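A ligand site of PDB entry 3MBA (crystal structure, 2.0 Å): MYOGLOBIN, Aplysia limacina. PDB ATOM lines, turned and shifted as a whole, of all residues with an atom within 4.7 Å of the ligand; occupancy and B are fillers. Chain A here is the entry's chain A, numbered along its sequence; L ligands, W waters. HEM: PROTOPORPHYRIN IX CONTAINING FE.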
ATOM      1  N   PHE A  29      32.244   3.583  22.498  1.00  0.00           N
ATOM      2  CA  PHE A  29      31.276   2.517  22.599  1.00  0.00           C
ATOM      3  C   PHE A  29      31.006   1.998  21.195  1.00  0.00           C
ATOM      4  O   PHE A  29      30.914   0.803  20.929  1.00  0.00           O
ATOM      5  CB  PHE A  29      29.943   3.005  23.216  1.00  0.00           C
ATOM      6  CG  PHE A  29      28.750   2.089  22.989  1.00  0.00           C
ATOM      7  CD1 PHE A  29      28.686   0.838  23.598  1.00  0.00           C
ATOM      8  CD2 PHE A  29      27.718   2.453  22.125  1.00  0.00           C
ATOM      9  CE1 PHE A  29      27.655  -0.083  23.373  1.00  0.00           C
ATOM     10  CE2 PHE A  29      26.686   1.546  21.900  1.00  0.00           C
ATOM     11  CZ  PHE A  29      26.613   0.293  22.525  1.00  0.00           C
ATOM     12  N   LEU A  33      31.921  -1.804  19.731  1.00  0.00           N
ATOM     13  CA  LEU A  33      30.881  -2.641  19.191  1.00  0.00           C
ATOM     14  C   LEU A  33      31.321  -3.192  17.844  1.00  0.00           C
ATOM     15  O   LEU A  33      31.259  -4.391  17.569  1.00  0.00           O
ATOM     16  CB  LEU A  33      29.557  -1.840  18.974  1.00  0.00           C
ATOM     17  CG  LEU A  33      28.365  -2.644  18.448  1.00  0.00           C
ATOM     18  CD1 LEU A  33      27.955  -3.741  19.407  1.00  0.00           C
ATOM     19  CD2 LEU A  33      27.196  -1.742  18.111  1.00  0.00           C
ATOM     20  N   SER A  40      27.736  -5.511  12.521  1.00  0.00           N
ATOM     21  CA  SER A  40      26.910  -4.397  12.939  1.00  0.00           C
ATOM     22  C   SER A  40      27.081  -3.128  12.165  1.00  0.00           C
ATOM     23  O   SER A  40      26.179  -2.331  11.958  1.00  0.00           O
ATOM     24  CB  SER A  40      26.903  -4.278  14.460  1.00  0.00           C
ATOM     25  OG  SER A  40      28.151  -3.688  14.734  1.00  0.00           O
ATOM     26  N   PHE A  43      24.789  -2.173   9.176  1.00  0.00           N
ATOM     27  CA  PHE A  43      23.433  -1.671   9.355  1.00  0.00           C
ATOM     28  C   PHE A  43      23.322  -0.176   9.186  1.00  0.00           C
ATOM     29  O   PHE A  43      22.275   0.374   8.825  1.00  0.00           O
ATOM     30  CB  PHE A  43      22.904  -2.029  10.731  1.00  0.00           C
ATOM     31  CG  PHE A  43      22.625  -3.500  10.818  1.00  0.00           C
ATOM     32  CD1 PHE A  43      21.362  -3.977  10.432  1.00  0.00           C
ATOM     33  CD2 PHE A  43      23.599  -4.406  11.227  1.00  0.00           C
ATOM     34  CE1 PHE A  43      21.095  -5.347  10.496  1.00  0.00           C
ATOM     35  CE2 PHE A  43      23.332  -5.768  11.298  1.00  0.00           C
ATOM     36  CZ  PHE A  43      22.080  -6.239  10.933  1.00  0.00           C
ATOM     37  N   PHE A  44      24.463   0.474   9.422  1.00  0.00           N
ATOM     38  CA  PHE A  44      24.540   1.921   9.306  1.00  0.00           C
ATOM     39  C   PHE A  44      24.863   2.318   7.899  1.00  0.00           C
ATOM     40  O   PHE A  44      25.806   1.839   7.320  1.00  0.00           O
ATOM     41  CB  PHE A  44      25.630   2.449  10.249  1.00  0.00           C
ATOM     42  CG  PHE A  44      25.300   2.348  11.690  1.00  0.00           C
ATOM     43  CD1 PHE A  44      24.722   3.455  12.336  1.00  0.00           C
ATOM     44  CD2 PHE A  44      25.532   1.210  12.461  1.00  0.00           C
ATOM     45  CE1 PHE A  44      24.427   3.354  13.696  1.00  0.00           C
ATOM     46  CE2 PHE A  44      25.278   1.110  13.832  1.00  0.00           C
ATOM     47  CZ  PHE A  44      24.698   2.206  14.449  1.00  0.00           C
ATOM     48  N   ALA A  45      24.043   3.191   7.370  1.00  0.00           N
ATOM     49  CA  ALA A  45      24.215   3.639   6.013  1.00  0.00           C
ATOM     50  C   ALA A  45      25.610   4.253   5.850  1.00  0.00           C
ATOM     51  O   ALA A  45      26.304   4.042   4.853  1.00  0.00           O
ATOM     52  CB  ALA A  45      23.133   4.698   5.764  1.00  0.00           C
ATOM     53  N   ASP A  46      25.975   5.031   6.865  1.00  0.00           N
ATOM     54  CA  ASP A  46      27.206   5.778   6.908  1.00  0.00           C
ATOM     55  C   ASP A  46      28.464   4.959   7.023  1.00  0.00           C
ATOM     56  O   ASP A  46      29.505   5.401   6.550  1.00  0.00           O
ATOM     57  CB  ASP A  46      27.165   6.777   8.067  1.00  0.00           C
ATOM     58  CG  ASP A  46      26.159   7.908   7.967  1.00  0.00           C
ATOM     59  OD1 ASP A  46      25.455   8.221   8.915  1.00  0.00           O
ATOM     60  OD2 ASP A  46      26.063   8.547   6.820  1.00  0.00           O
ATOM     61  N   VAL A  64      26.477  10.055  15.159  1.00  0.00           N
ATOM     62  CA  VAL A  64      25.984   8.713  15.456  1.00  0.00           C
ATOM     63  C   VAL A  64      26.130   8.290  16.932  1.00  0.00           C
ATOM     64  O   VAL A  64      25.186   7.838  17.638  1.00  0.00           O
ATOM     65  CB  VAL A  64      26.558   7.694  14.438  1.00  0.00           C
ATOM     66  CG1 VAL A  64      26.005   6.302  14.687  1.00  0.00           C
ATOM     67  CG2 VAL A  64      26.181   7.994  12.994  1.00  0.00           C
ATOM     68  N   ARG A  67      23.892  10.581  19.293  1.00  0.00           N
ATOM     69  CA  ARG A  67      22.470  10.299  19.244  1.00  0.00           C
ATOM     70  C   ARG A  67      22.199   9.031  20.032  1.00  0.00           C
ATOM     71  O   ARG A  67      21.184   8.827  20.667  1.00  0.00           O
ATOM     72  CB  ARG A  67      22.140  10.150  17.768  1.00  0.00           C
ATOM     73  CG  ARG A  67      22.402   8.713  17.311  1.00  0.00           C
ATOM     74  CD  ARG A  67      21.962   8.442  15.864  1.00  0.00           C
ATOM     75  NE  ARG A  67      22.048   7.023  15.500  1.00  0.00           N
ATOM     76  CZ  ARG A  67      22.020   6.766  14.207  1.00  0.00           C
ATOM     77  NH1 ARG A  67      21.900   7.802  13.364  1.00  0.00           N
ATOM     78  NH2 ARG A  67      22.099   5.509  13.754  1.00  0.00           N
ATOM     79  N   ILE A  68      23.118   8.090  20.073  1.00  0.00           N
ATOM     80  CA  ILE A  68      22.963   6.865  20.834  1.00  0.00           C
ATOM     81  C   ILE A  68      23.117   7.109  22.322  1.00  0.00           C
ATOM     82  O   ILE A  68      22.333   6.672  23.159  1.00  0.00           O
ATOM     83  CB  ILE A  68      23.977   5.798  20.412  1.00  0.00           C
ATOM     84  CG1 ILE A  68      23.680   5.227  19.014  1.00  0.00           C
ATOM     85  CG2 ILE A  68      24.127   4.666  21.446  1.00  0.00           C
ATOM     86  CD1 ILE A  68      24.696   4.193  18.509  1.00  0.00           C
ATOM     87  N   ARG A  71      20.050   9.117  23.814  1.00  0.00           N
ATOM     88  CA  ARG A  71      18.879   8.250  23.929  1.00  0.00           C
ATOM     89  C   ARG A  71      19.048   7.302  25.108  1.00  0.00           C
ATOM     90  O   ARG A  71      18.170   7.052  25.928  1.00  0.00           O
ATOM     91  CB  ARG A  71      18.474   7.582  22.605  1.00  0.00           C
ATOM     92  CG  ARG A  71      17.253   6.666  22.671  1.00  0.00           C
ATOM     93  CD  ARG A  71      15.958   7.461  22.991  1.00  0.00           C
ATOM     94  NE  ARG A  71      15.707   8.445  21.956  1.00  0.00           N
ATOM     95  CZ  ARG A  71      15.043   8.130  20.844  1.00  0.00           C
ATOM     96  NH1 ARG A  71      14.485   6.930  20.657  1.00  0.00           N
ATOM     97  NH2 ARG A  71      14.922   9.059  19.895  1.00  0.00           N
ATOM     98  N   LEU A  72      20.257   6.764  25.216  1.00  0.00           N
ATOM     99  CA  LEU A  72      20.548   5.817  26.271  1.00  0.00           C
ATOM    100  C   LEU A  72      20.367   6.425  27.645  1.00  0.00           C
ATOM    101  O   LEU A  72      19.928   5.774  28.598  1.00  0.00           O
ATOM    102  CB  LEU A  72      21.993   5.279  26.176  1.00  0.00           C
ATOM    103  CG  LEU A  72      22.176   3.770  26.090  1.00  0.00           C
ATOM    104  CD1 LEU A  72      23.553   3.394  26.585  1.00  0.00           C
ATOM    105  CD2 LEU A  72      21.150   2.961  26.858  1.00  0.00           C
ATOM    106  N   PHE A  92      11.354   3.225  20.145  1.00  0.00           N
ATOM    107  CA  PHE A  92      12.716   2.795  19.835  1.00  0.00           C
ATOM    108  C   PHE A  92      12.684   1.614  18.890  1.00  0.00           C
ATOM    109  O   PHE A  92      13.384   1.590  17.861  1.00  0.00           O
ATOM    110  CB  PHE A  92      13.414   2.346  21.139  1.00  0.00           C
ATOM    111  CG  PHE A  92      14.861   1.992  20.962  1.00  0.00           C
ATOM    112  CD1 PHE A  92      15.807   3.005  20.788  1.00  0.00           C
ATOM    113  CD2 PHE A  92      15.271   0.653  20.961  1.00  0.00           C
ATOM    114  CE1 PHE A  92      17.162   2.720  20.644  1.00  0.00           C
ATOM    115  CE2 PHE A  92      16.625   0.349  20.794  1.00  0.00           C
ATOM    116  CZ  PHE A  92      17.552   1.380  20.658  1.00  0.00           C
ATOM    117  N   HIS A  96      14.098   1.408  14.838  1.00  0.00           N
ATOM    118  CA  HIS A  96      15.117   0.452  14.452  1.00  0.00           C
ATOM    119  C   HIS A  96      14.717  -0.651  13.498  1.00  0.00           C
ATOM    120  O   HIS A  96      15.465  -0.958  12.596  1.00  0.00           O
ATOM    121  CB  HIS A  96      15.735  -0.205  15.713  1.00  0.00           C
ATOM    122  CG  HIS A  96      16.737   0.771  16.264  1.00  0.00           C
ATOM    123  ND1 HIS A  96      16.346   1.822  17.077  1.00  0.00           N
ATOM    124  CD2 HIS A  96      18.081   0.853  16.037  1.00  0.00           C
ATOM    125  CE1 HIS A  96      17.443   2.511  17.319  1.00  0.00           C
ATOM    126  NE2 HIS A  96      18.501   1.962  16.720  1.00  0.00           N
ATOM    127  N   PHE A  99      14.859   0.225  10.059  1.00  0.00           N
ATOM    128  CA  PHE A  99      16.150   0.340   9.405  1.00  0.00           C
ATOM    129  C   PHE A  99      16.763  -1.019   9.152  1.00  0.00           C
ATOM    130  O   PHE A  99      17.826  -1.049   8.549  1.00  0.00           O
ATOM    131  CB  PHE A  99      17.053   1.119  10.356  1.00  0.00           C
ATOM    132  CG  PHE A  99      16.501   2.494  10.633  1.00  0.00           C
ATOM    133  CD1 PHE A  99      16.108   3.328   9.586  1.00  0.00           C
ATOM    134  CD2 PHE A  99      16.452   3.022  11.942  1.00  0.00           C
ATOM    135  CE1 PHE A  99      15.652   4.624   9.865  1.00  0.00           C
ATOM    136  CE2 PHE A  99      16.017   4.318  12.233  1.00  0.00           C
ATOM    137  CZ  PHE A  99      15.595   5.109  11.171  1.00  0.00           C
ATOM    138  N   VAL A 101      17.398  -3.394  11.699  1.00  0.00           N
ATOM    139  CA  VAL A 101      18.058  -3.825  12.921  1.00  0.00           C
ATOM    140  C   VAL A 101      17.068  -4.671  13.735  1.00  0.00           C
ATOM    141  O   VAL A 101      15.916  -4.322  13.952  1.00  0.00           O
ATOM    142  CB  VAL A 101      18.553  -2.560  13.665  1.00  0.00           C
ATOM    143  CG1 VAL A 101      19.544  -2.957  14.771  1.00  0.00           C
ATOM    144  CG2 VAL A 101      19.200  -1.528  12.733  1.00  0.00           C
ATOM    145  N   GLN A 105      21.074  -7.929  17.060  1.00  0.00           N
ATOM    146  CA  GLN A 105      22.055  -6.867  17.149  1.00  0.00           C
ATOM    147  C   GLN A 105      22.080  -6.291  18.547  1.00  0.00           C
ATOM    148  O   GLN A 105      23.111  -5.753  18.976  1.00  0.00           O
ATOM    149  CB  GLN A 105      21.728  -5.689  16.209  1.00  0.00           C
ATOM    150  CG  GLN A 105      22.077  -6.060  14.745  1.00  0.00           C
ATOM    151  CD  GLN A 105      21.203  -7.203  14.274  1.00  0.00           C
ATOM    152  OE1 GLN A 105      19.956  -7.104  14.206  1.00  0.00           O
ATOM    153  NE2 GLN A 105      21.835  -8.328  13.935  1.00  0.00           N
ATOM    154  N   PHE A 106      20.945  -6.421  19.252  1.00  0.00           N
ATOM    155  CA  PHE A 106      20.804  -5.947  20.635  1.00  0.00           C
ATOM    156  C   PHE A 106      21.336  -6.974  21.625  1.00  0.00           C
ATOM    157  O   PHE A 106      21.806  -6.526  22.675  1.00  0.00           O
ATOM    158  CB  PHE A 106      19.454  -5.322  20.999  1.00  0.00           C
ATOM    159  CG  PHE A 106      19.440  -3.908  20.434  1.00  0.00           C
ATOM    160  CD1 PHE A 106      19.859  -2.834  21.214  1.00  0.00           C
ATOM    161  CD2 PHE A 106      18.984  -3.615  19.144  1.00  0.00           C
ATOM    162  CE1 PHE A 106      19.816  -1.552  20.685  1.00  0.00           C
ATOM    163  CE2 PHE A 106      18.951  -2.332  18.601  1.00  0.00           C
ATOM    164  CZ  PHE A 106      19.381  -1.258  19.394  1.00  0.00           C
ATOM    165  N   VAL A 109      25.044  -6.055  21.756  1.00  0.00           N
ATOM    166  CA  VAL A 109      25.240  -4.871  22.603  1.00  0.00           C
ATOM    167  C   VAL A 109      25.204  -5.304  24.064  1.00  0.00           C
ATOM    168  O   VAL A 109      26.056  -5.069  24.922  1.00  0.00           O
ATOM    169  CB  VAL A 109      24.175  -3.810  22.325  1.00  0.00           C
ATOM    170  CG1 VAL A 109      24.297  -2.692  23.351  1.00  0.00           C
ATOM    171  CG2 VAL A 109      24.295  -3.234  20.923  1.00  0.00           C
ATOM    172  N   PHE A 135      18.729  -4.068  28.807  1.00  0.00           N
ATOM    173  CA  PHE A 135      18.914  -4.468  27.411  1.00  0.00           C
ATOM    174  C   PHE A 135      17.948  -5.603  27.053  1.00  0.00           C
ATOM    175  O   PHE A 135      17.599  -5.738  25.885  1.00  0.00           O
ATOM    176  CB  PHE A 135      20.365  -4.877  27.095  1.00  0.00           C
ATOM    177  CG  PHE A 135      21.149  -3.641  26.834  1.00  0.00           C
ATOM    178  CD1 PHE A 135      22.173  -3.247  27.724  1.00  0.00           C
ATOM    179  CD2 PHE A 135      20.834  -2.840  25.721  1.00  0.00           C
ATOM    180  CE1 PHE A 135      22.848  -2.058  27.439  1.00  0.00           C
ATOM    181  CE2 PHE A 135      21.541  -1.672  25.454  1.00  0.00           C
ATOM    182  CZ  PHE A 135      22.526  -1.288  26.339  1.00  0.00           C
HETATM  183  CHA HEM L   1      19.163   5.392  14.436  1.00  0.00           C
HETATM  184  CHB HEM L   1      19.639   5.092  19.277  1.00  0.00           C
HETATM  185  CHC HEM L   1      21.845   0.825  18.827  1.00  0.00           C
HETATM  186  CHD HEM L   1      21.260   1.125  14.003  1.00  0.00           C
HETATM  187  C1A HEM L   1      18.937   5.601  15.788  1.00  0.00           C
HETATM  188  C2A HEM L   1      18.302   6.765  16.386  1.00  0.00           C
HETATM  189  C3A HEM L   1      18.562   6.728  17.706  1.00  0.00           C
HETATM  190  C4A HEM L   1      19.249   5.472  18.002  1.00  0.00           C
HETATM  191  CMA HEM L   1      18.170   7.701  18.841  1.00  0.00           C
HETATM  192  CAA HEM L   1      17.654   7.916  15.569  1.00  0.00           C
HETATM  193  CBA HEM L   1      18.546   9.161  15.698  1.00  0.00           C
HETATM  194  CGA HEM L   1      18.342  10.291  14.746  1.00  0.00           C
HETATM  195  O1A HEM L   1      17.644  11.252  15.137  1.00  0.00           O
HETATM  196  O2A HEM L   1      18.889  10.200  13.632  1.00  0.00           O
HETATM  197  C1B HEM L   1      20.254   3.900  19.610  1.00  0.00           C
HETATM  198  C2B HEM L   1      20.621   3.478  20.948  1.00  0.00           C
HETATM  199  C3B HEM L   1      21.273   2.290  20.824  1.00  0.00           C
HETATM  200  C4B HEM L   1      21.193   1.918  19.407  1.00  0.00           C
HETATM  201  CMB HEM L   1      20.001   4.074  22.205  1.00  0.00           C
HETATM  202  CAB HEM L   1      21.740   1.348  21.966  1.00  0.00           C
HETATM  203  CBB HEM L   1      22.893   0.741  22.216  1.00  0.00           C
HETATM  204  C1C HEM L   1      21.949   0.610  17.456  1.00  0.00           C
HETATM  205  C2C HEM L   1      22.479  -0.617  16.863  1.00  0.00           C
HETATM  206  C3C HEM L   1      22.312  -0.489  15.527  1.00  0.00           C
HETATM  207  C4C HEM L   1      21.714   0.820  15.263  1.00  0.00           C
HETATM  208  CMC HEM L   1      23.049  -1.775  17.713  1.00  0.00           C
HETATM  209  CAC HEM L   1      22.805  -1.347  14.369  1.00  0.00           C
HETATM  210  CBC HEM L   1      23.101  -2.548  14.862  1.00  0.00           C
HETATM  211  C1D HEM L   1      20.619   2.285  13.698  1.00  0.00           C
HETATM  212  C2D HEM L   1      20.309   2.719  12.334  1.00  0.00           C
HETATM  213  C3D HEM L   1      19.795   3.950  12.458  1.00  0.00           C
HETATM  214  C4D HEM L   1      19.614   4.191  13.901  1.00  0.00           C
HETATM  215  CMD HEM L   1      20.712   1.911  11.081  1.00  0.00           C
HETATM  216  CAD HEM L   1      19.203   4.814  11.321  1.00  0.00           C
HETATM  217  CBD HEM L   1      19.932   6.113  10.911  1.00  0.00           C
HETATM  218  CGD HEM L   1      21.326   5.768  10.433  1.00  0.00           C
HETATM  219  O1D HEM L   1      21.446   4.996   9.460  1.00  0.00           O
HETATM  220  O2D HEM L   1      22.285   6.267  11.072  1.00  0.00           O
HETATM  221  NA  HEM L   1      19.579   4.899  16.782  1.00  0.00           N
HETATM  222  NB  HEM L   1      20.766   3.013  18.677  1.00  0.00           N
HETATM  223  NC  HEM L   1      21.373   1.394  16.469  1.00  0.00           N
HETATM  224  ND  HEM L   1      20.303   3.233  14.626  1.00  0.00           N
HETATM  225 FE   HEM L   1      20.489   3.017  16.546  1.00  0.00          FE
HETATM  226  O   HOH W   1      22.972   9.014  10.428  1.00  0.00           O
HETATM  227  O   HOH W   2      20.871   2.619   8.270  1.00  0.00           O
HETATM  228  O   HOH W   3      18.019  11.929  17.693  1.00  0.00           O
HETATM  229  O   HOH W   4      24.597   5.636   9.432  1.00  0.00           O
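The backbone carbonyl oxygen of Phe 92 is in hydrogen-bond range of a ring nitrogen (ND1) of His 96, 3.1 Å away. O of His 96 is in hydrogen-bond range of N of Val 101, 3.2 Å away.
Merely in contact with the ligand: Phe 29 (3.8 Å), Phe 43 (3.1 Å), Phe 44 (3.4 Å), Ala 45 (3.8 Å), Ile 68 (3.6 Å), Arg 71 (3.7 Å), Phe 92 (3.5 Å), Phe 99 (3.3 Å), Val 101 (3.6 Å), Gln 105 (3.7 Å), Phe 106 (3.3 Å) and Val 109 (3.7 Å). Within 4 Å of the ligand: Phe 29, Phe 43, Phe 44, Ala 45, Arg 67, Ile 68, Arg 71, Phe 92, His 96, Phe 99, Val 101, Gln 105, Phe 106 and Val 109.
A ring nitrogen (NE2) of His 96 is bound to an iron atom (FE) of the ligand (2.3 Å). An oxygen (O2D) of the ligand is in salt-bridge range of the guanidinium group (NH1) of Arg 67 (2.8 Å).
Water W2 lies within hydrogen-bond range of O of Phe 43 (2.7 Å), O1D of the ligand (2.7 Å) and N of Ala 45 (3.3 Å). Water W1 lies within hydrogen-bond range of O2D of the ligand (2.9 Å), OD1 of Asp 46 (3.0 Å) and NH1 of Arg 67 (3.4 Å). Water W4 lies within hydrogen-bond range of OD1 of Asp 46, O2D of the ligand and N of Ala 45.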
